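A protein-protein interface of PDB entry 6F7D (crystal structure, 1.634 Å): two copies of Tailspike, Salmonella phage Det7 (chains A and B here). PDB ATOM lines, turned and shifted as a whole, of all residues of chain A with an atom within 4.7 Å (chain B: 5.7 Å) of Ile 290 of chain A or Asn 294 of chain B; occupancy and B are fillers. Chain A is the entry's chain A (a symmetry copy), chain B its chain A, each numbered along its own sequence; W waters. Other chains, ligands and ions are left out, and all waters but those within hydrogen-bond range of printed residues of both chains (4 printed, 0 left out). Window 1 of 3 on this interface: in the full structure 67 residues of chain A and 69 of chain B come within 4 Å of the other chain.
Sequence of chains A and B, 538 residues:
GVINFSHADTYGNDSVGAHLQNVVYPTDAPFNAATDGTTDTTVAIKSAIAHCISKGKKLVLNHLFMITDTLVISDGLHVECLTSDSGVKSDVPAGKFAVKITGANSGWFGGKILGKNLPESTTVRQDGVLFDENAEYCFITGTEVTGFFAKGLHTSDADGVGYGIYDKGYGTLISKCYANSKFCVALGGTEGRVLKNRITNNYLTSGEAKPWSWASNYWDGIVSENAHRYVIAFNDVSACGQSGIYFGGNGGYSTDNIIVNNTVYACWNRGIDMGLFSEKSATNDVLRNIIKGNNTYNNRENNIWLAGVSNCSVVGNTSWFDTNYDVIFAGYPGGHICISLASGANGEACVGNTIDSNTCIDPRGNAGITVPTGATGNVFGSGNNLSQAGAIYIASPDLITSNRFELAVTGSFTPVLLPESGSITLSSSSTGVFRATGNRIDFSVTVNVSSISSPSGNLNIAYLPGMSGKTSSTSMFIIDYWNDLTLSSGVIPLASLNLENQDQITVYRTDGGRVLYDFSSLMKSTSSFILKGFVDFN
Ile 258 of chain A touches Asn 262 of chain B (CD1 to O, 3.9 Å).
Ile 258 of chain A touches Gly 293 of chain B (CD1 to O, 3.7 Å).
O of Arg 288 of chain A touches ND2 of Asn 295 of chain B, 3.6 Å away.
Ile 290 of chain A touches Gly 293 of chain B (CD1 to O, 3.99 Å).
O of Asn 294 of chain B touches CD1 of Ile 290 of chain A (3.5 Å).
Ile 290 of chain A touches Thr 318 of chain B.
Lys 292 of chain B touches Lys 292 of chain A.
NZ of Lys 292 of chain A touches CA of Gly 316 of chain B, 3.8 Å away.
Lys 292 of chain B touches its own counterpart, Lys 292 of chain A.
Positions printed for both chains: 259, 291 and 292.
Of the 10 pairs that touch across the chains among the printed residues, 1 has its exchanged pair printed and touching as well.
Water W1 lies within hydrogen-bond range of OG1 of Thr 318 of chain B (2.6 Å) and O of Asn 289 of chain A (3.1 Å).
Water W3 lies within hydrogen-bond range of the backbone carbonyl oxygen of Arg 288 of chain A, the side-chain amide nitrogen of Asn 295 of chain B and the backbone carbonyl oxygen of Asn 257 of chain A.
Water W2 lies within hydrogen-bond range of the side-chain hydroxyl of Thr 318 of chain B, the backbone carbonyl oxygen of Gly 316 of chain B, the side-chain hydroxyl of Ser 313 of chain A and the backbone carbonyl oxygen of Asn 317 of chain B.
Water W4 lies within hydrogen-bond range of OD1 of Asn 261 of chain B and NZ of Lys 292 of chain A.
O of Ile 232 of chain B lies within hydrogen-bond range of ND2 of Asn 262 of chain B.
N of Asn 262 of chain B lies within hydrogen-bond range of OD1 of Asn 294 of chain B, 2.9 Å away.
The backbone NH (N) of Val 264 of chain B lies within hydrogen-bond range of the backbone carbonyl oxygen (O) of Asn 295 of chain B.
The backbone NH (N) of Gly 293 of chain B sits at hydrogen-bond distance from the side-chain amide oxygen (OD1) of Asn 317 of chain B.
The backbone carbonyl oxygen (O) of Asn 257 of chain A lies within hydrogen-bond range of the backbone NH (N) of Ile 290 of chain A (2.9 Å).
O of Ile 259 of chain A lies within hydrogen-bond range of N of Lys 292 of chain A, 3.0 Å away.
Of the 9 printed residues of chain A, 4 touch a printed residue of chain B.
Printed residues of chain A that touch a printed residue of chain B: Ile 258, Arg 288, Ile 290 and Lys 292.
Hydrophobic or aromatic side chains of chain A within 4 Å of the printed part of chain B: Ile 258 and Ile 290.
Along chain A the printed residues that touch a printed residue of chain B span positions 258 to 292.
Printed residues of chain B that touch a printed residue of chain A: Asn 262, Lys 292, Gly 293, Asn 294, Asn 295, Val 315, Gly 316 and Thr 318.
Among the printed residues, 10 pairs touch across the chains.
Among the printed residues, no Asp or Glu carboxylate lies within 4 Å of a Lys or Arg side-chain nitrogen of the other chain.
O of Val 315 of chain B sits at hydrogen-bond distance from NZ of Lys 292 of chain A (3.4 Å).
NZ of Lys 292 of chain A sits close to N of Gly 293 of chain B (3.3 Å).
Of the printed residues of chain B, Ile 290 of chain A touches Gly 293, Asn 294 and Thr 318.
Of the printed residues of chain A, Asn 294 of chain B touches Ile 290 (3.5 Å).
Of the printed residues of chain A, Asn 295 of chain B touches Arg 288.
Of the printed residues of chain B, Lys 292 of chain A touches Lys 292 (3.5 Å), Gly 293 (3.3 Å), Val 315 (3.4 Å) and Gly 316 (3.8 Å).
Printed residues of chain A within 4 Å of Gly 293 of chain B: Ile 258, Ile 290 and Lys 292.
Asn 317 of chain B touches none of the printed residues of chain A.
The nearest printed residue of chain B that does not touch Ile 290 of chain A is Gly 316 of chain B (4.2 Å).
The nearest printed residue of chain A that does not touch Asn 294 of chain B is Ile 258 of chain A (4.7 Å).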
ATOM      1  N   ASN A 257      16.108  33.937  24.247  1.00  0.00           N
ATOM      2  CA  ASN A 257      14.713  34.051  24.666  1.00  0.00           C
ATOM      3  C   ASN A 257      14.033  32.683  24.534  1.00  0.00           C
ATOM      4  O   ASN A 257      14.453  31.856  23.714  1.00  0.00           O
ATOM      5  CB  ASN A 257      14.010  35.089  23.792  1.00  0.00           C
ATOM      6  CG  ASN A 257      14.680  36.442  23.896  1.00  0.00           C
ATOM      7  OD1 ASN A 257      14.592  37.085  24.942  1.00  0.00           O
ATOM      8  ND2 ASN A 257      15.458  36.821  22.880  1.00  0.00           N
ATOM      9  N   ILE A 258      12.977  32.473  25.321  1.00  0.00           N
ATOM     10  CA  ILE A 258      12.288  31.175  25.389  1.00  0.00           C
ATOM     11  C   ILE A 258      10.799  31.452  25.159  1.00  0.00           C
ATOM     12  O   ILE A 258      10.168  32.164  25.949  1.00  0.00           O
ATOM     13  CB  ILE A 258      12.535  30.482  26.738  1.00  0.00           C
ATOM     14  CG1 ILE A 258      14.035  30.240  26.946  1.00  0.00           C
ATOM     15  CG2 ILE A 258      11.804  29.145  26.830  1.00  0.00           C
ATOM     16  CD1 ILE A 258      14.357  29.673  28.372  1.00  0.00           C
ATOM     17  N   ILE A 259      10.268  30.972  24.036  1.00  0.00           N
ATOM     18  CA  ILE A 259       8.905  31.269  23.585  1.00  0.00           C
ATOM     19  C   ILE A 259       8.157  29.938  23.620  1.00  0.00           C
ATOM     20  O   ILE A 259       8.371  29.080  22.746  1.00  0.00           O
ATOM     21  CB  ILE A 259       8.932  31.871  22.178  1.00  0.00           C
ATOM     22  CG1 ILE A 259       9.711  33.200  22.177  1.00  0.00           C
ATOM     23  CG2 ILE A 259       7.489  32.101  21.638  1.00  0.00           C
ATOM     24  CD1 ILE A 259      11.185  33.101  21.758  1.00  0.00           C
ATOM     25  N   ARG A 288      19.996  31.879  19.352  1.00  0.00           N
ATOM     26  CA  ARG A 288      19.809  31.018  20.528  1.00  0.00           C
ATOM     27  C   ARG A 288      18.437  31.206  21.163  1.00  0.00           C
ATOM     28  O   ARG A 288      18.300  31.135  22.380  1.00  0.00           O
ATOM     29  CB  ARG A 288      20.901  31.233  21.585  1.00  0.00           C
ATOM     30  CG  ARG A 288      22.294  30.801  21.065  1.00  0.00           C
ATOM     31  CD  ARG A 288      23.378  31.017  22.167  1.00  0.00           C
ATOM     32  NE  ARG A 288      23.281  32.352  22.752  1.00  0.00           N
ATOM     33  CZ  ARG A 288      23.991  33.417  22.353  1.00  0.00           C
ATOM     34  NH1 ARG A 288      24.889  33.298  21.366  1.00  0.00           N
ATOM     35  NH2 ARG A 288      23.826  34.605  22.960  1.00  0.00           N
ATOM     36  N   ASN A 289      17.420  31.425  20.343  1.00  0.00           N
ATOM     37  CA  ASN A 289      16.058  31.448  20.867  1.00  0.00           C
ATOM     38  C   ASN A 289      15.417  30.074  20.755  1.00  0.00           C
ATOM     39  O   ASN A 289      15.681  29.323  19.814  1.00  0.00           O
ATOM     40  CB  ASN A 289      15.229  32.500  20.133  1.00  0.00           C
ATOM     41  CG  ASN A 289      15.853  33.888  20.297  1.00  0.00           C
ATOM     42  OD1 ASN A 289      16.080  34.331  21.395  1.00  0.00           O
ATOM     43  ND2 ASN A 289      16.290  34.470  19.193  1.00  0.00           N
ATOM     44  N   ILE A 290      14.552  29.773  21.723  1.00  0.00           N
ATOM     45  CA  ILE A 290      13.878  28.480  21.834  1.00  0.00           C
ATOM     46  C   ILE A 290      12.400  28.710  21.545  1.00  0.00           C
ATOM     47  O   ILE A 290      11.766  29.519  22.234  1.00  0.00           O
ATOM     48  CB  ILE A 290      14.068  27.892  23.248  1.00  0.00           C
ATOM     49  CG1 ILE A 290      15.545  27.528  23.495  1.00  0.00           C
ATOM     50  CG2 ILE A 290      13.173  26.631  23.433  1.00  0.00           C
ATOM     51  CD1 ILE A 290      15.914  27.061  24.953  1.00  0.00           C
ATOM     52  N   ILE A 291      11.839  27.971  20.570  1.00  0.00           N
ATOM     53  CA  ILE A 291      10.406  28.037  20.211  1.00  0.00           C
ATOM     54  C   ILE A 291       9.842  26.646  20.457  1.00  0.00           C
ATOM     55  O   ILE A 291      10.121  25.738  19.671  1.00  0.00           O
ATOM     56  CB  ILE A 291      10.183  28.464  18.748  1.00  0.00           C
ATOM     57  CG1 ILE A 291      10.734  29.875  18.515  1.00  0.00           C
ATOM     58  CG2 ILE A 291       8.647  28.447  18.412  1.00  0.00           C
ATOM     59  CD1 ILE A 291      10.784  30.244  16.995  1.00  0.00           C
ATOM     60  N   LYS A 292       9.098  26.447  21.558  1.00  0.00           N
ATOM     61  CA  LYS A 292       8.747  25.069  21.958  1.00  0.00           C
ATOM     62  C   LYS A 292       7.304  24.958  22.398  1.00  0.00           C
ATOM     63  O   LYS A 292       6.817  25.796  23.159  1.00  0.00           O
ATOM     64  CB  LYS A 292       9.627  24.595  23.122  1.00  0.00           C
ATOM     65  CG  LYS A 292      10.711  23.720  22.724  1.00  0.00           C
ATOM     66  CD  LYS A 292      11.442  23.168  23.945  1.00  0.00           C
ATOM     67  CE  LYS A 292      11.241  21.659  24.076  1.00  0.00           C
ATOM     68  NZ  LYS A 292      11.700  21.367  25.391  1.00  0.00           N
ATOM     69  N   SER A 313      15.969  27.085  18.032  1.00  0.00           N
ATOM     70  CA  SER A 313      15.336  25.771  17.994  1.00  0.00           C
ATOM     71  C   SER A 313      13.826  25.916  17.838  1.00  0.00           C
ATOM     72  O   SER A 313      13.212  26.877  18.317  1.00  0.00           O
ATOM     73  CB  SER A 313      15.659  24.967  19.266  1.00  0.00           C
ATOM     74  OG  SER A 313      15.145  25.635  20.437  1.00  0.00           O
ATOM     75  N   ILE B 232      10.215  23.332  38.537  1.00  0.00           N
ATOM     76  CA  ILE B 232      11.155  24.448  38.698  1.00  0.00           C
ATOM     77  C   ILE B 232      11.138  25.130  37.336  1.00  0.00           C
ATOM     78  O   ILE B 232      11.631  24.562  36.360  1.00  0.00           O
ATOM     79  CB  ILE B 232      12.564  23.968  39.088  1.00  0.00           C
ATOM     80  CG1 ILE B 232      12.502  23.164  40.418  1.00  0.00           C
ATOM     81  CG2 ILE B 232      13.540  25.166  39.229  1.00  0.00           C
ATOM     82  CD1 ILE B 232      13.833  22.704  40.827  1.00  0.00           C
ATOM     83  N   ILE B 245      21.192  24.704  39.619  1.00  0.00           N
ATOM     84  CA  ILE B 245      20.057  23.878  40.044  1.00  0.00           C
ATOM     85  C   ILE B 245      20.600  22.474  40.252  1.00  0.00           C
ATOM     86  O   ILE B 245      20.983  21.812  39.275  1.00  0.00           O
ATOM     87  CB  ILE B 245      18.942  23.855  38.994  1.00  0.00           C
ATOM     88  CG1 ILE B 245      18.436  25.276  38.748  1.00  0.00           C
ATOM     89  CG2 ILE B 245      17.769  23.020  39.481  1.00  0.00           C
ATOM     90  CD1 ILE B 245      17.375  25.358  37.593  1.00  0.00           C
ATOM     91  N   ILE B 259      12.235  20.361  35.496  1.00  0.00           N
ATOM     92  CA  ILE B 259      13.079  21.560  35.497  1.00  0.00           C
ATOM     93  C   ILE B 259      12.989  22.131  34.084  1.00  0.00           C
ATOM     94  O   ILE B 259      13.592  21.579  33.149  1.00  0.00           O
ATOM     95  CB  ILE B 259      14.517  21.195  35.874  1.00  0.00           C
ATOM     96  CG1 ILE B 259      14.566  20.604  37.295  1.00  0.00           C
ATOM     97  CG2 ILE B 259      15.452  22.437  35.783  1.00  0.00           C
ATOM     98  CD1 ILE B 259      14.553  19.070  37.374  1.00  0.00           C
ATOM     99  N   VAL B 260      12.195  23.200  33.876  1.00  0.00           N
ATOM    100  CA  VAL B 260      11.797  23.608  32.529  1.00  0.00           C
ATOM    101  C   VAL B 260      11.861  25.117  32.369  1.00  0.00           C
ATOM    102  O   VAL B 260      11.460  25.876  33.261  1.00  0.00           O
ATOM    103  CB  VAL B 260      10.366  23.131  32.177  1.00  0.00           C
ATOM    104  CG1 VAL B 260      10.371  21.663  31.875  1.00  0.00           C
ATOM    105  CG2 VAL B 260       9.390  23.486  33.281  1.00  0.00           C
ATOM    106  N   ASN B 261      12.352  25.559  31.200  1.00  0.00           N
ATOM    107  CA  ASN B 261      12.244  26.947  30.771  1.00  0.00           C
ATOM    108  C   ASN B 261      12.906  27.894  31.768  1.00  0.00           C
ATOM    109  O   ASN B 261      12.367  28.963  32.069  1.00  0.00           O
ATOM    110  CB  ASN B 261      10.763  27.343  30.535  1.00  0.00           C
ATOM    111  CG  ASN B 261      10.049  26.359  29.604  1.00  0.00           C
ATOM    112  OD1 ASN B 261      10.656  25.758  28.679  1.00  0.00           O
ATOM    113  ND2 ASN B 261       8.800  26.138  29.879  1.00  0.00           N
ATOM    114  N   ASN B 262      14.078  27.505  32.287  1.00  0.00           N
ATOM    115  CA  ASN B 262      14.882  28.382  33.135  1.00  0.00           C
ATOM    116  C   ASN B 262      16.092  28.856  32.354  1.00  0.00           C
ATOM    117  O   ASN B 262      16.481  28.233  31.373  1.00  0.00           O
ATOM    118  CB  ASN B 262      15.395  27.651  34.393  1.00  0.00           C
ATOM    119  CG  ASN B 262      14.284  27.013  35.199  1.00  0.00           C
ATOM    120  OD1 ASN B 262      13.657  27.655  36.013  1.00  0.00           O
ATOM    121  ND2 ASN B 262      14.070  25.720  34.998  1.00  0.00           N
ATOM    122  N   THR B 263      16.688  29.957  32.810  1.00  0.00           N
ATOM    123  CA  THR B 263      17.997  30.393  32.309  1.00  0.00           C
ATOM    124  C   THR B 263      19.004  30.157  33.418  1.00  0.00           C
ATOM    125  O   THR B 263      18.758  30.563  34.549  1.00  0.00           O
ATOM    126  CB  THR B 263      17.992  31.890  31.933  1.00  0.00           C
ATOM    127  OG1 THR B 263      17.536  32.665  33.057  1.00  0.00           O
ATOM    128  CG2 THR B 263      16.986  32.139  30.845  1.00  0.00           C
ATOM    129  N   VAL B 264      20.100  29.460  33.125  1.00  0.00           N
ATOM    130  CA  VAL B 264      21.041  29.088  34.178  1.00  0.00           C
ATOM    131  C   VAL B 264      22.440  29.360  33.653  1.00  0.00           C
ATOM    132  O   VAL B 264      22.850  28.750  32.659  1.00  0.00           O
ATOM    133  CB  VAL B 264      20.921  27.603  34.605  1.00  0.00           C
ATOM    134  CG1 VAL B 264      21.834  27.359  35.818  1.00  0.00           C
ATOM    135  CG2 VAL B 264      19.464  27.212  34.963  1.00  0.00           C
ATOM    136  N   ILE B 272      22.806  22.891  35.489  1.00  0.00           N
ATOM    137  CA  ILE B 272      21.808  21.972  36.020  1.00  0.00           C
ATOM    138  C   ILE B 272      22.558  20.686  36.310  1.00  0.00           C
ATOM    139  O   ILE B 272      23.183  20.120  35.410  1.00  0.00           O
ATOM    140  CB  ILE B 272      20.653  21.756  35.025  1.00  0.00           C
ATOM    141  CG1 ILE B 272      19.984  23.104  34.760  1.00  0.00           C
ATOM    142  CG2 ILE B 272      19.643  20.750  35.592  1.00  0.00           C
ATOM    143  CD1 ILE B 272      18.834  23.055  33.702  1.00  0.00           C
ATOM    144  N   ILE B 291      14.519  17.529  32.296  1.00  0.00           N
ATOM    145  CA  ILE B 291      15.251  18.795  32.074  1.00  0.00           C
ATOM    146  C   ILE B 291      14.900  19.245  30.665  1.00  0.00           C
ATOM    147  O   ILE B 291      15.395  18.650  29.704  1.00  0.00           O
ATOM    148  CB  ILE B 291      16.774  18.632  32.232  1.00  0.00           C
ATOM    149  CG1 ILE B 291      17.119  18.198  33.660  1.00  0.00           C
ATOM    150  CG2 ILE B 291      17.495  19.992  31.915  1.00  0.00           C
ATOM    151  CD1 ILE B 291      18.613  17.753  33.797  1.00  0.00           C
ATOM    152  N   LYS B 292      14.019  20.248  30.518  1.00  0.00           N
ATOM    153  CA  LYS B 292      13.470  20.543  29.178  1.00  0.00           C
ATOM    154  C   LYS B 292      13.415  22.029  28.904  1.00  0.00           C
ATOM    155  O   LYS B 292      12.985  22.807  29.758  1.00  0.00           O
ATOM    156  CB  LYS B 292      12.045  19.990  29.036  1.00  0.00           C
ATOM    157  CG  LYS B 292      11.968  18.746  28.297  1.00  0.00           C
ATOM    158  CD  LYS B 292      10.513  18.342  28.064  1.00  0.00           C
ATOM    159  CE  LYS B 292      10.155  18.401  26.579  1.00  0.00           C
ATOM    160  NZ  LYS B 292       8.734  18.313  26.570  1.00  0.00           N
ATOM    161  N   GLY B 293      13.835  22.426  27.705  1.00  0.00           N
ATOM    162  CA  GLY B 293      13.592  23.789  27.276  1.00  0.00           C
ATOM    163  C   GLY B 293      14.304  24.853  28.094  1.00  0.00           C
ATOM    164  O   GLY B 293      13.815  25.987  28.176  1.00  0.00           O
ATOM    165  N   ASN B 294      15.459  24.531  28.673  1.00  0.00           N
ATOM    166  CA  ASN B 294      16.255  25.505  29.414  1.00  0.00           C
ATOM    167  C   ASN B 294      17.345  26.075  28.517  1.00  0.00           C
ATOM    168  O   ASN B 294      17.727  25.466  27.515  1.00  0.00           O
ATOM    169  CB  ASN B 294      16.933  24.844  30.634  1.00  0.00           C
ATOM    170  CG  ASN B 294      15.947  24.223  31.587  1.00  0.00           C
ATOM    171  OD1 ASN B 294      15.418  24.920  32.418  1.00  0.00           O
ATOM    172  ND2 ASN B 294      15.754  22.903  31.512  1.00  0.00           N
ATOM    173  N   ASN B 295      17.830  27.264  28.884  1.00  0.00           N
ATOM    174  CA  ASN B 295      18.992  27.885  28.237  1.00  0.00           C
ATOM    175  C   ASN B 295      20.080  27.904  29.311  1.00  0.00           C
ATOM    176  O   ASN B 295      19.933  28.589  30.339  1.00  0.00           O
ATOM    177  CB  ASN B 295      18.630  29.294  27.736  1.00  0.00           C
ATOM    178  CG  ASN B 295      19.752  29.921  26.951  1.00  0.00           C
ATOM    179  OD1 ASN B 295      20.897  29.851  27.367  1.00  0.00           O
ATOM    180  ND2 ASN B 295      19.437  30.468  25.766  1.00  0.00           N
ATOM    181  N   THR B 296      21.136  27.103  29.108  1.00  0.00           N
ATOM    182  CA  THR B 296      22.202  26.982  30.101  1.00  0.00           C
ATOM    183  C   THR B 296      23.518  27.369  29.429  1.00  0.00           C
ATOM    184  O   THR B 296      23.854  26.803  28.389  1.00  0.00           O
ATOM    185  CB  THR B 296      22.312  25.535  30.656  1.00  0.00           C
ATOM    186  OG1 THR B 296      22.564  24.601  29.585  1.00  0.00           O
ATOM    187  CG2 THR B 296      21.011  25.091  31.360  1.00  0.00           C
ATOM    188  N   VAL B 315      15.858  17.268  27.148  1.00  0.00           N
ATOM    189  CA  VAL B 315      15.202  17.401  25.839  1.00  0.00           C
ATOM    190  C   VAL B 315      14.995  18.877  25.524  1.00  0.00           C
ATOM    191  O   VAL B 315      14.409  19.619  26.324  1.00  0.00           O
ATOM    192  CB  VAL B 315      13.842  16.657  25.800  1.00  0.00           C
ATOM    193  CG1 VAL B 315      13.116  16.872  24.457  1.00  0.00           C
ATOM    194  CG2 VAL B 315      14.066  15.161  26.023  1.00  0.00           C
ATOM    195  N   GLY B 316      15.428  19.287  24.339  1.00  0.00           N
ATOM    196  CA  GLY B 316      15.044  20.605  23.874  1.00  0.00           C
ATOM    197  C   GLY B 316      15.708  21.782  24.570  1.00  0.00           C
ATOM    198  O   GLY B 316      15.177  22.910  24.511  1.00  0.00           O
ATOM    199  N   ASN B 317      16.870  21.573  25.181  1.00  0.00           N
ATOM    200  CA  ASN B 317      17.640  22.637  25.831  1.00  0.00           C
ATOM    201  C   ASN B 317      18.636  23.223  24.864  1.00  0.00           C
ATOM    202  O   ASN B 317      19.074  22.551  23.932  1.00  0.00           O
ATOM    203  CB  ASN B 317      18.416  22.079  27.045  1.00  0.00           C
ATOM    204  CG  ASN B 317      17.508  21.401  28.037  1.00  0.00           C
ATOM    205  OD1 ASN B 317      16.883  22.054  28.870  1.00  0.00           O
ATOM    206  ND2 ASN B 317      17.410  20.082  27.944  1.00  0.00           N
ATOM    207  N   THR B 318      18.980  24.490  25.083  1.00  0.00           N
ATOM    208  CA  THR B 318      20.072  25.113  24.348  1.00  0.00           C
ATOM    209  C   THR B 318      21.197  25.344  25.337  1.00  0.00           C
ATOM    210  O   THR B 318      21.014  26.085  26.305  1.00  0.00           O
ATOM    211  CB  THR B 318      19.602  26.423  23.718  1.00  0.00           C
ATOM    212  OG1 THR B 318      18.625  26.108  22.706  1.00  0.00           O
ATOM    213  CG2 THR B 318      20.790  27.137  23.050  1.00  0.00           C
ATOM    214  N   SER B 319      22.342  24.702  25.095  1.00  0.00           N
ATOM    215  CA  SER B 319      23.452  24.655  26.064  1.00  0.00           C
ATOM    216  C   SER B 319      24.678  25.148  25.317  1.00  0.00           C
ATOM    217  O   SER B 319      24.966  24.629  24.236  1.00  0.00           O
ATOM    218  CB  SER B 319      23.674  23.225  26.551  1.00  0.00           C
ATOM    219  OG  SER B 319      24.790  23.188  27.429  1.00  0.00           O
HETATM  220  O   HOH W   1      18.153  27.790  20.738  1.00  0.00           O
HETATM  221  O   HOH W   2      16.522  24.329  22.527  1.00  0.00           O
HETATM  222  O   HOH W   3      16.936  30.375  24.602  1.00  0.00           O
HETATM  223  O   HOH W   4       9.748  23.358  27.010  1.00  0.00           O
